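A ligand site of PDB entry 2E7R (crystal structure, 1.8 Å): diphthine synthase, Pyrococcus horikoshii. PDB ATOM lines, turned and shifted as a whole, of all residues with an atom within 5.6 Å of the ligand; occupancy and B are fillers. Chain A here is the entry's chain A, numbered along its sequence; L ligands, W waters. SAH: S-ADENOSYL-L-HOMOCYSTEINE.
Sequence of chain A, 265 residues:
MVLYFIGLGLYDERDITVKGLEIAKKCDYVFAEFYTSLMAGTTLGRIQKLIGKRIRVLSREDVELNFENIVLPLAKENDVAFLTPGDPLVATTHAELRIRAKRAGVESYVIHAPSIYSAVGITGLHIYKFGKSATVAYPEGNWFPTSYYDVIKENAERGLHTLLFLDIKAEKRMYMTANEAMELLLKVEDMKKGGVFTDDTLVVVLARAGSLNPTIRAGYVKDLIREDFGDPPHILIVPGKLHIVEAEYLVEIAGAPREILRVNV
SD of the ligand sits close to O of Thr 36 (3.7 Å). Merely in contact with the ligand: Pro 85 (3.9 Å), Gly 86 (3.7 Å), Ala 91 (3.8 Å), Thr 92 (3.7 Å), Phe 165 (3.6 Å), Leu 206 (3.7 Å), Arg 208 (3.5 Å), Pro 233 (3.4 Å) and Ile 235 (3.7 Å). Hydrophobic or aromatic side chains that line the ligand: Leu 10, Val 90, Ala 91, Ile 116, Phe 165, Leu 166, Ala 209, Pro 233 and Ile 235. 19 residues have an atom within 4 Å of the ligand: Leu 10, Thr 36, Ser 37, Pro 85, Gly 86, Asp 87, Val 90, Ala 91, Thr 92, Ser 115, Ile 116, Phe 165, Leu 166, Leu 206, Arg 208, Ala 209, Pro 233, His 234 and Ile 235.
The side-chain hydroxyl (OG1) of Thr 92 lies within hydrogen-bond range of the backbone carbonyl oxygen (O) of Pro 88, at 2.8 Å. The side-chain carboxylate of Asp 87 sits at hydrogen-bond distance from the backbone NH of Leu 89 (2.9 Å). The backbone carbonyl oxygen (O) of Pro 233 is in hydrogen-bond range of the backbone NH (N) of Arg 208 (3.0 Å). The backbone NH of Tyr 117 sits close to the side-chain hydroxyl of Ser 115. O of Leu 206 is in hydrogen-bond range of N of Ile 235 (3.0 Å).
Water W3 lies within hydrogen-bond range of a nitrogen (N) of the ligand, the side-chain hydroxyl of Thr 36 and the backbone carbonyl oxygen of Pro 85. Water W4 lies within hydrogen-bond range of O3' of the ligand (2.9 Å) and O of Asp 167 (3.0 Å).
O of the ligand lies within hydrogen-bond range of OG of Ser 115 (2.7 Å). The backbone carbonyl oxygen of Leu 166 sits at hydrogen-bond distance from an oxygen (O3') of the ligand (2.6 Å). N1 of the ligand sits at hydrogen-bond distance from N of Ala 209 (3.0 Å). A nitrogen (N7) of the ligand sits close to the side-chain hydroxyl of Ser 37, 3.5 Å away. The backbone carbonyl oxygen (O) of Leu 10 lies within hydrogen-bond range of a nitrogen (N6) of the ligand, at 3.2 Å. A nitrogen (N) of the ligand lies within hydrogen-bond range of the backbone carbonyl oxygen (O) of Val 90 (2.6 Å). The backbone carbonyl oxygen (O) of Asp 87 sits at hydrogen-bond distance from a nitrogen (N) of the ligand (2.9 Å). An oxygen (O) of the ligand sits at hydrogen-bond distance from the backbone NH (N) of Asp 87 (2.9 Å). An oxygen (O2') of the ligand lies within hydrogen-bond range of the backbone carbonyl oxygen (O) of His 234 (2.7 Å). O2' of the ligand sits at hydrogen-bond distance from N of Leu 166 (2.9 Å). An oxygen (OXT) of the ligand lies within hydrogen-bond range of the backbone NH (N) of Ile 116, 3.0 Å away. The backbone carbonyl oxygen of Ala 209 lies within hydrogen-bond range of a nitrogen (N6) of the ligand.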
ATOM      1  N   LEU A  10       6.525  17.331  32.748  1.00  0.00           N
ATOM      2  CA  LEU A  10       7.792  17.241  32.034  1.00  0.00           C
ATOM      3  C   LEU A  10       8.027  16.335  30.839  1.00  0.00           C
ATOM      4  O   LEU A  10       8.611  16.759  29.842  1.00  0.00           O
ATOM      5  CB  LEU A  10       8.886  16.915  33.047  1.00  0.00           C
ATOM      6  CG  LEU A  10       9.044  17.757  34.307  1.00  0.00           C
ATOM      7  CD1 LEU A  10       9.889  17.008  35.326  1.00  0.00           C
ATOM      8  CD2 LEU A  10       9.688  19.084  33.952  1.00  0.00           C
ATOM      9  N   TYR A  11       7.580  15.087  30.930  1.00  0.00           N
ATOM     10  CA  TYR A  11       7.907  14.120  29.900  1.00  0.00           C
ATOM     11  C   TYR A  11       6.790  13.302  29.249  1.00  0.00           C
ATOM     12  O   TYR A  11       6.754  13.177  28.023  1.00  0.00           O
ATOM     13  CB  TYR A  11       8.955  13.187  30.518  1.00  0.00           C
ATOM     14  CG  TYR A  11       9.535  12.151  29.589  1.00  0.00           C
ATOM     15  CD1 TYR A  11      10.406  12.510  28.556  1.00  0.00           C
ATOM     16  CD2 TYR A  11       9.247  10.800  29.783  1.00  0.00           C
ATOM     17  CE1 TYR A  11      10.985  11.533  27.735  1.00  0.00           C
ATOM     18  CE2 TYR A  11       9.817   9.828  28.961  1.00  0.00           C
ATOM     19  CZ  TYR A  11      10.678  10.193  27.947  1.00  0.00           C
ATOM     20  OH  TYR A  11      11.245   9.223  27.154  1.00  0.00           O
ATOM     21  N   THR A  36       5.220  25.491  23.397  1.00  0.00           N
ATOM     22  CA  THR A  36       6.086  26.108  24.394  1.00  0.00           C
ATOM     23  C   THR A  36       7.163  25.159  24.895  1.00  0.00           C
ATOM     24  O   THR A  36       8.197  25.593  25.407  1.00  0.00           O
ATOM     25  CB  THR A  36       5.279  26.633  25.608  1.00  0.00           C
ATOM     26  OG1 THR A  36       4.521  25.566  26.178  1.00  0.00           O
ATOM     27  CG2 THR A  36       4.351  27.758  25.184  1.00  0.00           C
ATOM     28  N   SER A  37       6.924  23.865  24.758  1.00  0.00           N
ATOM     29  CA  SER A  37       7.895  22.865  25.190  1.00  0.00           C
ATOM     30  C   SER A  37       7.643  21.540  24.500  1.00  0.00           C
ATOM     31  O   SER A  37       6.634  21.366  23.816  1.00  0.00           O
ATOM     32  CB  SER A  37       7.838  22.689  26.715  1.00  0.00           C
ATOM     33  OG  SER A  37       8.891  21.851  27.137  1.00  0.00           O
ATOM     34  N   LEU A  38       8.566  20.599  24.702  1.00  0.00           N
ATOM     35  CA  LEU A  38       8.456  19.275  24.107  1.00  0.00           C
ATOM     36  C   LEU A  38       8.311  18.164  25.139  1.00  0.00           C
ATOM     37  O   LEU A  38       9.172  18.002  26.007  1.00  0.00           O
ATOM     38  CB  LEU A  38       9.695  18.980  23.250  1.00  0.00           C
ATOM     39  CG  LEU A  38       9.809  17.548  22.706  1.00  0.00           C
ATOM     40  CD1 LEU A  38       8.686  17.274  21.703  1.00  0.00           C
ATOM     41  CD2 LEU A  38      11.162  17.342  22.038  1.00  0.00           C
ATOM     42  N   PRO A  85       2.424  21.901  28.246  1.00  0.00           N
ATOM     43  CA  PRO A  85       3.514  21.062  28.742  1.00  0.00           C
ATOM     44  C   PRO A  85       4.044  21.724  30.023  1.00  0.00           C
ATOM     45  O   PRO A  85       3.856  22.924  30.209  1.00  0.00           O
ATOM     46  CB  PRO A  85       4.546  21.129  27.611  1.00  0.00           C
ATOM     47  CG  PRO A  85       3.718  21.394  26.389  1.00  0.00           C
ATOM     48  CD  PRO A  85       2.713  22.401  26.890  1.00  0.00           C
ATOM     49  N   GLY A  86       4.686  20.942  30.891  1.00  0.00           N
ATOM     50  CA  GLY A  86       5.226  21.480  32.129  1.00  0.00           C
ATOM     51  C   GLY A  86       4.204  22.219  32.965  1.00  0.00           C
ATOM     52  O   GLY A  86       3.072  21.756  33.099  1.00  0.00           O
ATOM     53  N   ASP A  87       4.605  23.343  33.551  1.00  0.00           N
ATOM     54  CA  ASP A  87       3.702  24.162  34.335  1.00  0.00           C
ATOM     55  C   ASP A  87       3.226  25.231  33.359  1.00  0.00           C
ATOM     56  O   ASP A  87       4.028  25.856  32.666  1.00  0.00           O
ATOM     57  CB  ASP A  87       4.436  24.801  35.518  1.00  0.00           C
ATOM     58  CG  ASP A  87       3.523  25.673  36.359  1.00  0.00           C
ATOM     59  OD1 ASP A  87       3.101  26.748  35.862  1.00  0.00           O
ATOM     60  OD2 ASP A  87       3.220  25.291  37.505  1.00  0.00           O
ATOM     61  N   PRO A  88       1.901  25.465  33.283  1.00  0.00           N
ATOM     62  CA  PRO A  88       1.352  26.451  32.354  1.00  0.00           C
ATOM     63  C   PRO A  88       1.843  27.894  32.409  1.00  0.00           C
ATOM     64  O   PRO A  88       1.810  28.584  31.401  1.00  0.00           O
ATOM     65  CB  PRO A  88      -0.158  26.336  32.589  1.00  0.00           C
ATOM     66  CG  PRO A  88      -0.247  25.943  34.031  1.00  0.00           C
ATOM     67  CD  PRO A  88       0.860  24.921  34.167  1.00  0.00           C
ATOM     68  N   LEU A  89       2.318  28.332  33.575  1.00  0.00           N
ATOM     69  CA  LEU A  89       2.772  29.714  33.700  1.00  0.00           C
ATOM     70  C   LEU A  89       4.269  29.927  33.830  1.00  0.00           C
ATOM     71  O   LEU A  89       4.721  31.023  34.182  1.00  0.00           O
ATOM     72  CB  LEU A  89       2.067  30.375  34.897  1.00  0.00           C
ATOM     73  CG  LEU A  89       0.544  30.248  34.920  1.00  0.00           C
ATOM     74  CD1 LEU A  89      -0.003  30.890  36.185  1.00  0.00           C
ATOM     75  CD2 LEU A  89      -0.043  30.905  33.692  1.00  0.00           C
ATOM     76  N   VAL A  90       5.055  28.891  33.549  1.00  0.00           N
ATOM     77  CA  VAL A  90       6.499  28.996  33.649  1.00  0.00           C
ATOM     78  C   VAL A  90       7.184  29.123  32.286  1.00  0.00           C
ATOM     79  O   VAL A  90       7.082  28.239  31.447  1.00  0.00           O
ATOM     80  CB  VAL A  90       7.106  27.775  34.366  1.00  0.00           C
ATOM     81  CG1 VAL A  90       8.638  27.837  34.327  1.00  0.00           C
ATOM     82  CG2 VAL A  90       6.623  27.719  35.808  1.00  0.00           C
ATOM     83  N   ALA A  91       7.891  30.230  32.081  1.00  0.00           N
ATOM     84  CA  ALA A  91       8.597  30.449  30.816  1.00  0.00           C
ATOM     85  C   ALA A  91       7.654  30.431  29.627  1.00  0.00           C
ATOM     86  O   ALA A  91       8.008  29.958  28.543  1.00  0.00           O
ATOM     87  CB  ALA A  91       9.696  29.400  30.640  1.00  0.00           C
ATOM     88  N   THR A  92       6.447  30.930  29.841  1.00  0.00           N
ATOM     89  CA  THR A  92       5.439  31.165  28.823  1.00  0.00           C
ATOM     90  C   THR A  92       4.817  32.536  29.043  1.00  0.00           C
ATOM     91  O   THR A  92       5.054  33.201  30.040  1.00  0.00           O
ATOM     92  CB  THR A  92       4.357  30.075  28.956  1.00  0.00           C
ATOM     93  OG1 THR A  92       3.489  30.403  30.043  1.00  0.00           O
ATOM     94  CG2 THR A  92       4.996  28.709  29.221  1.00  0.00           C
ATOM     95  N   PRO A 114       4.791  19.434  37.320  1.00  0.00           N
ATOM     96  CA  PRO A 114       6.261  19.499  37.396  1.00  0.00           C
ATOM     97  C   PRO A 114       6.817  20.395  36.289  1.00  0.00           C
ATOM     98  O   PRO A 114       6.424  20.272  35.135  1.00  0.00           O
ATOM     99  CB  PRO A 114       6.681  18.043  37.198  1.00  0.00           C
ATOM    100  CG  PRO A 114       5.518  17.272  37.739  1.00  0.00           C
ATOM    101  CD  PRO A 114       4.321  18.037  37.245  1.00  0.00           C
ATOM    102  N   SER A 115       7.733  21.286  36.672  1.00  0.00           N
ATOM    103  CA  SER A 115       8.343  22.228  35.730  1.00  0.00           C
ATOM    104  C   SER A 115       9.839  22.005  35.663  1.00  0.00           C
ATOM    105  O   SER A 115      10.455  21.618  36.647  1.00  0.00           O
ATOM    106  CB  SER A 115       8.063  23.661  36.185  1.00  0.00           C
ATOM    107  OG  SER A 115       8.778  24.593  35.396  1.00  0.00           O
ATOM    108  N   ILE A 116      10.434  22.258  34.494  1.00  0.00           N
ATOM    109  CA  ILE A 116      11.865  22.089  34.367  1.00  0.00           C
ATOM    110  C   ILE A 116      12.585  23.075  35.287  1.00  0.00           C
ATOM    111  O   ILE A 116      13.696  22.818  35.744  1.00  0.00           O
ATOM    112  CB  ILE A 116      12.325  22.327  32.903  1.00  0.00           C
ATOM    113  CG1 ILE A 116      13.805  21.949  32.751  1.00  0.00           C
ATOM    114  CG2 ILE A 116      12.094  23.777  32.506  1.00  0.00           C
ATOM    115  CD1 ILE A 116      14.087  20.479  33.033  1.00  0.00           C
ATOM    116  N   TYR A 117      11.930  24.205  35.568  1.00  0.00           N
ATOM    117  CA  TYR A 117      12.516  25.230  36.431  1.00  0.00           C
ATOM    118  C   TYR A 117      12.888  24.684  37.811  1.00  0.00           C
ATOM    119  O   TYR A 117      13.887  25.116  38.390  1.00  0.00           O
ATOM    120  CB  TYR A 117      11.533  26.407  36.543  1.00  0.00           C
ATOM    121  CG  TYR A 117      12.032  27.584  37.349  1.00  0.00           C
ATOM    122  CD1 TYR A 117      13.108  28.361  36.929  1.00  0.00           C
ATOM    123  CD2 TYR A 117      11.385  27.958  38.527  1.00  0.00           C
ATOM    124  CE1 TYR A 117      13.534  29.479  37.650  1.00  0.00           C
ATOM    125  CE2 TYR A 117      11.781  29.071  39.265  1.00  0.00           C
ATOM    126  CZ  TYR A 117      12.858  29.824  38.817  1.00  0.00           C
ATOM    127  OH  TYR A 117      13.233  30.939  39.542  1.00  0.00           O
ATOM    128  N   LEU A 164      19.596  27.838  31.637  1.00  0.00           N
ATOM    129  CA  LEU A 164      19.391  28.275  30.272  1.00  0.00           C
ATOM    130  C   LEU A 164      18.364  27.413  29.543  1.00  0.00           C
ATOM    131  O   LEU A 164      18.636  26.256  29.212  1.00  0.00           O
ATOM    132  CB  LEU A 164      20.713  28.258  29.499  1.00  0.00           C
ATOM    133  CG  LEU A 164      21.830  29.148  30.055  1.00  0.00           C
ATOM    134  CD1 LEU A 164      23.139  28.841  29.328  1.00  0.00           C
ATOM    135  CD2 LEU A 164      21.452  30.606  29.894  1.00  0.00           C
ATOM    136  N   PHE A 165      17.184  27.984  29.313  1.00  0.00           N
ATOM    137  CA  PHE A 165      16.140  27.299  28.582  1.00  0.00           C
ATOM    138  C   PHE A 165      16.669  27.301  27.159  1.00  0.00           C
ATOM    139  O   PHE A 165      17.342  28.254  26.757  1.00  0.00           O
ATOM    140  CB  PHE A 165      14.843  28.108  28.639  1.00  0.00           C
ATOM    141  CG  PHE A 165      14.240  28.202  30.009  1.00  0.00           C
ATOM    142  CD1 PHE A 165      13.428  27.182  30.501  1.00  0.00           C
ATOM    143  CD2 PHE A 165      14.477  29.309  30.821  1.00  0.00           C
ATOM    144  CE1 PHE A 165      12.865  27.263  31.775  1.00  0.00           C
ATOM    145  CE2 PHE A 165      13.917  29.412  32.094  1.00  0.00           C
ATOM    146  CZ  PHE A 165      13.111  28.377  32.567  1.00  0.00           C
ATOM    147  N   LEU A 166      16.409  26.244  26.393  1.00  0.00           N
ATOM    148  CA  LEU A 166      16.890  26.181  25.018  1.00  0.00           C
ATOM    149  C   LEU A 166      15.729  26.395  24.044  1.00  0.00           C
ATOM    150  O   LEU A 166      14.590  26.029  24.323  1.00  0.00           O
ATOM    151  CB  LEU A 166      17.594  24.841  24.774  1.00  0.00           C
ATOM    152  CG  LEU A 166      18.757  24.591  25.740  1.00  0.00           C
ATOM    153  CD1 LEU A 166      19.549  23.363  25.309  1.00  0.00           C
ATOM    154  CD2 LEU A 166      19.672  25.820  25.802  1.00  0.00           C
ATOM    155  N   ASP A 167      16.033  27.002  22.905  1.00  0.00           N
ATOM    156  CA  ASP A 167      15.008  27.331  21.920  1.00  0.00           C
ATOM    157  C   ASP A 167      14.241  26.144  21.348  1.00  0.00           C
ATOM    158  O   ASP A 167      14.718  25.006  21.341  1.00  0.00           O
ATOM    159  CB  ASP A 167      15.632  28.136  20.775  1.00  0.00           C
ATOM    160  CG  ASP A 167      14.640  29.092  20.122  1.00  0.00           C
ATOM    161  OD1 ASP A 167      13.464  29.128  20.547  1.00  0.00           O
ATOM    162  OD2 ASP A 167      15.050  29.818  19.190  1.00  0.00           O
ATOM    163  N   ILE A 168      13.037  26.438  20.869  1.00  0.00           N
ATOM    164  CA  ILE A 168      12.180  25.440  20.266  1.00  0.00           C
ATOM    165  C   ILE A 168      11.342  26.067  19.154  1.00  0.00           C
ATOM    166  O   ILE A 168      10.808  27.169  19.308  1.00  0.00           O
ATOM    167  CB  ILE A 168      11.235  24.784  21.318  1.00  0.00           C
ATOM    168  CG1 ILE A 168      10.206  23.886  20.610  1.00  0.00           C
ATOM    169  CG2 ILE A 168      10.527  25.856  22.129  1.00  0.00           C
ATOM    170  CD1 ILE A 168       9.316  23.089  21.555  1.00  0.00           C
ATOM    171  N   LEU A 206      20.983  18.605  31.345  1.00  0.00           N
ATOM    172  CA  LEU A 206      19.889  17.756  31.817  1.00  0.00           C
ATOM    173  C   LEU A 206      18.998  17.538  30.614  1.00  0.00           C
ATOM    174  O   LEU A 206      18.429  18.483  30.057  1.00  0.00           O
ATOM    175  CB  LEU A 206      19.089  18.455  32.931  1.00  0.00           C
ATOM    176  CG  LEU A 206      17.859  17.681  33.424  1.00  0.00           C
ATOM    177  CD1 LEU A 206      18.280  16.296  33.958  1.00  0.00           C
ATOM    178  CD2 LEU A 206      17.158  18.471  34.513  1.00  0.00           C
ATOM    179  N   ALA A 207      18.872  16.282  30.195  1.00  0.00           N
ATOM    180  CA  ALA A 207      18.054  15.946  29.037  1.00  0.00           C
ATOM    181  C   ALA A 207      16.921  15.015  29.408  1.00  0.00           C
ATOM    182  O   ALA A 207      17.115  14.024  30.118  1.00  0.00           O
ATOM    183  CB  ALA A 207      18.925  15.307  27.947  1.00  0.00           C
ATOM    184  N   ARG A 208      15.722  15.353  28.927  1.00  0.00           N
ATOM    185  CA  ARG A 208      14.509  14.584  29.160  1.00  0.00           C
ATOM    186  C   ARG A 208      14.164  14.415  30.643  1.00  0.00           C
ATOM    187  O   ARG A 208      13.876  13.309  31.105  1.00  0.00           O
ATOM    188  CB  ARG A 208      14.631  13.209  28.483  1.00  0.00           C
ATOM    189  CG  ARG A 208      14.880  13.297  26.974  1.00  0.00           C
ATOM    190  CD  ARG A 208      15.062  11.917  26.354  1.00  0.00           C
ATOM    191  NE  ARG A 208      16.091  11.162  27.070  1.00  0.00           N
ATOM    192  CZ  ARG A 208      17.385  11.437  27.055  1.00  0.00           C
ATOM    193  NH1 ARG A 208      17.846  12.458  26.344  1.00  0.00           N
ATOM    194  NH2 ARG A 208      18.230  10.716  27.780  1.00  0.00           N
ATOM    195  N   ALA A 209      14.184  15.520  31.370  1.00  0.00           N
ATOM    196  CA  ALA A 209      13.824  15.481  32.784  1.00  0.00           C
ATOM    197  C   ALA A 209      12.390  14.975  32.817  1.00  0.00           C
ATOM    198  O   ALA A 209      11.618  15.248  31.913  1.00  0.00           O
ATOM    199  CB  ALA A 209      13.900  16.885  33.390  1.00  0.00           C
ATOM    200  N   GLY A 210      12.042  14.220  33.858  1.00  0.00           N
ATOM    201  CA  GLY A 210      10.695  13.694  33.943  1.00  0.00           C
ATOM    202  C   GLY A 210      10.678  12.212  33.588  1.00  0.00           C
ATOM    203  O   GLY A 210       9.857  11.460  34.094  1.00  0.00           O
ATOM    204  N   PRO A 233      13.829  17.071  24.871  1.00  0.00           N
ATOM    205  CA  PRO A 233      14.408  18.395  25.113  1.00  0.00           C
ATOM    206  C   PRO A 233      15.638  18.388  26.033  1.00  0.00           C
ATOM    207  O   PRO A 233      15.825  17.482  26.838  1.00  0.00           O
ATOM    208  CB  PRO A 233      13.249  19.167  25.721  1.00  0.00           C
ATOM    209  CG  PRO A 233      12.580  18.110  26.552  1.00  0.00           C
ATOM    210  CD  PRO A 233      12.570  16.906  25.630  1.00  0.00           C
ATOM    211  N   HIS A 234      16.457  19.421  25.884  1.00  0.00           N
ATOM    212  CA  HIS A 234      17.664  19.596  26.690  1.00  0.00           C
ATOM    213  C   HIS A 234      17.613  20.950  27.366  1.00  0.00           C
ATOM    214  O   HIS A 234      16.952  21.881  26.891  1.00  0.00           O
ATOM    215  CB  HIS A 234      18.929  19.616  25.819  1.00  0.00           C
ATOM    216  CG  HIS A 234      19.231  18.327  25.106  1.00  0.00           C
ATOM    217  ND1 HIS A 234      20.354  18.164  24.320  1.00  0.00           N
ATOM    218  CD2 HIS A 234      18.564  17.152  25.057  1.00  0.00           C
ATOM    219  CE1 HIS A 234      20.372  16.948  23.824  1.00  0.00           C
ATOM    220  NE2 HIS A 234      19.300  16.311  24.256  1.00  0.00           N
ATOM    221  N   ILE A 235      18.317  21.063  28.484  1.00  0.00           N
ATOM    222  CA  ILE A 235      18.429  22.336  29.162  1.00  0.00           C
ATOM    223  C   ILE A 235      19.909  22.413  29.550  1.00  0.00           C
ATOM    224  O   ILE A 235      20.537  21.387  29.835  1.00  0.00           O
ATOM    225  CB  ILE A 235      17.500  22.415  30.397  1.00  0.00           C
ATOM    226  CG1 ILE A 235      17.361  23.877  30.836  1.00  0.00           C
ATOM    227  CG2 ILE A 235      18.017  21.555  31.527  1.00  0.00           C
ATOM    228  CD1 ILE A 235      16.002  24.218  31.395  1.00  0.00           C
HETATM  229  N   SAH L   1       6.384  25.745  31.034  1.00  0.00           N
HETATM  230  CA  SAH L   1       7.531  24.786  30.758  1.00  0.00           C
HETATM  231  CB  SAH L   1       8.778  25.373  30.135  1.00  0.00           C
HETATM  232  CG  SAH L   1       8.658  26.101  28.813  1.00  0.00           C
HETATM  233  SD  SAH L   1      10.372  26.482  28.273  1.00  0.00           S
HETATM  234  C   SAH L   1       7.889  24.084  32.124  1.00  0.00           C
HETATM  235  O   SAH L   1       7.249  24.397  33.146  1.00  0.00           O
HETATM  236  OXT SAH L   1       8.835  23.203  32.093  1.00  0.00           O
HETATM  237  C5' SAH L   1      10.689  25.080  27.276  1.00  0.00           C
HETATM  238  C4' SAH L   1      12.219  24.702  27.362  1.00  0.00           C
HETATM  239  O4' SAH L   1      12.480  24.216  28.706  1.00  0.00           O
HETATM  240  C3' SAH L   1      12.650  23.619  26.430  1.00  0.00           C
HETATM  241  O3' SAH L   1      12.974  24.155  25.157  1.00  0.00           O
HETATM  242  C2' SAH L   1      13.824  22.995  27.216  1.00  0.00           C
HETATM  243  O2' SAH L   1      15.032  23.731  27.035  1.00  0.00           O
HETATM  244  C1' SAH L   1      13.330  22.981  28.674  1.00  0.00           C
HETATM  245  N9  SAH L   1      12.603  21.897  29.038  1.00  0.00           N
HETATM  246  C8  SAH L   1      11.246  21.650  29.196  1.00  0.00           C
HETATM  247  N7  SAH L   1      10.939  20.439  29.571  1.00  0.00           N
HETATM  248  C5  SAH L   1      12.200  19.781  29.684  1.00  0.00           C
HETATM  249  C6  SAH L   1      12.535  18.431  30.055  1.00  0.00           C
HETATM  250  N6  SAH L   1      11.638  17.505  30.392  1.00  0.00           N
HETATM  251  N1  SAH L   1      13.882  18.160  30.055  1.00  0.00           N
HETATM  252  C2  SAH L   1      14.841  19.070  29.717  1.00  0.00           C
HETATM  253  N3  SAH L   1      14.554  20.365  29.353  1.00  0.00           N
HETATM  254  C4  SAH L   1      13.217  20.654  29.363  1.00  0.00           C
HETATM  255  O   HOH W   1       7.792  19.720  28.474  1.00  0.00           O
HETATM  256  O   HOH W   2       8.345  20.638  30.750  1.00  0.00           O
HETATM  257  O   HOH W   3       5.191  24.906  28.734  1.00  0.00           O
HETATM  258  O   HOH W   4      13.723  22.662  22.842  1.00  0.00           O
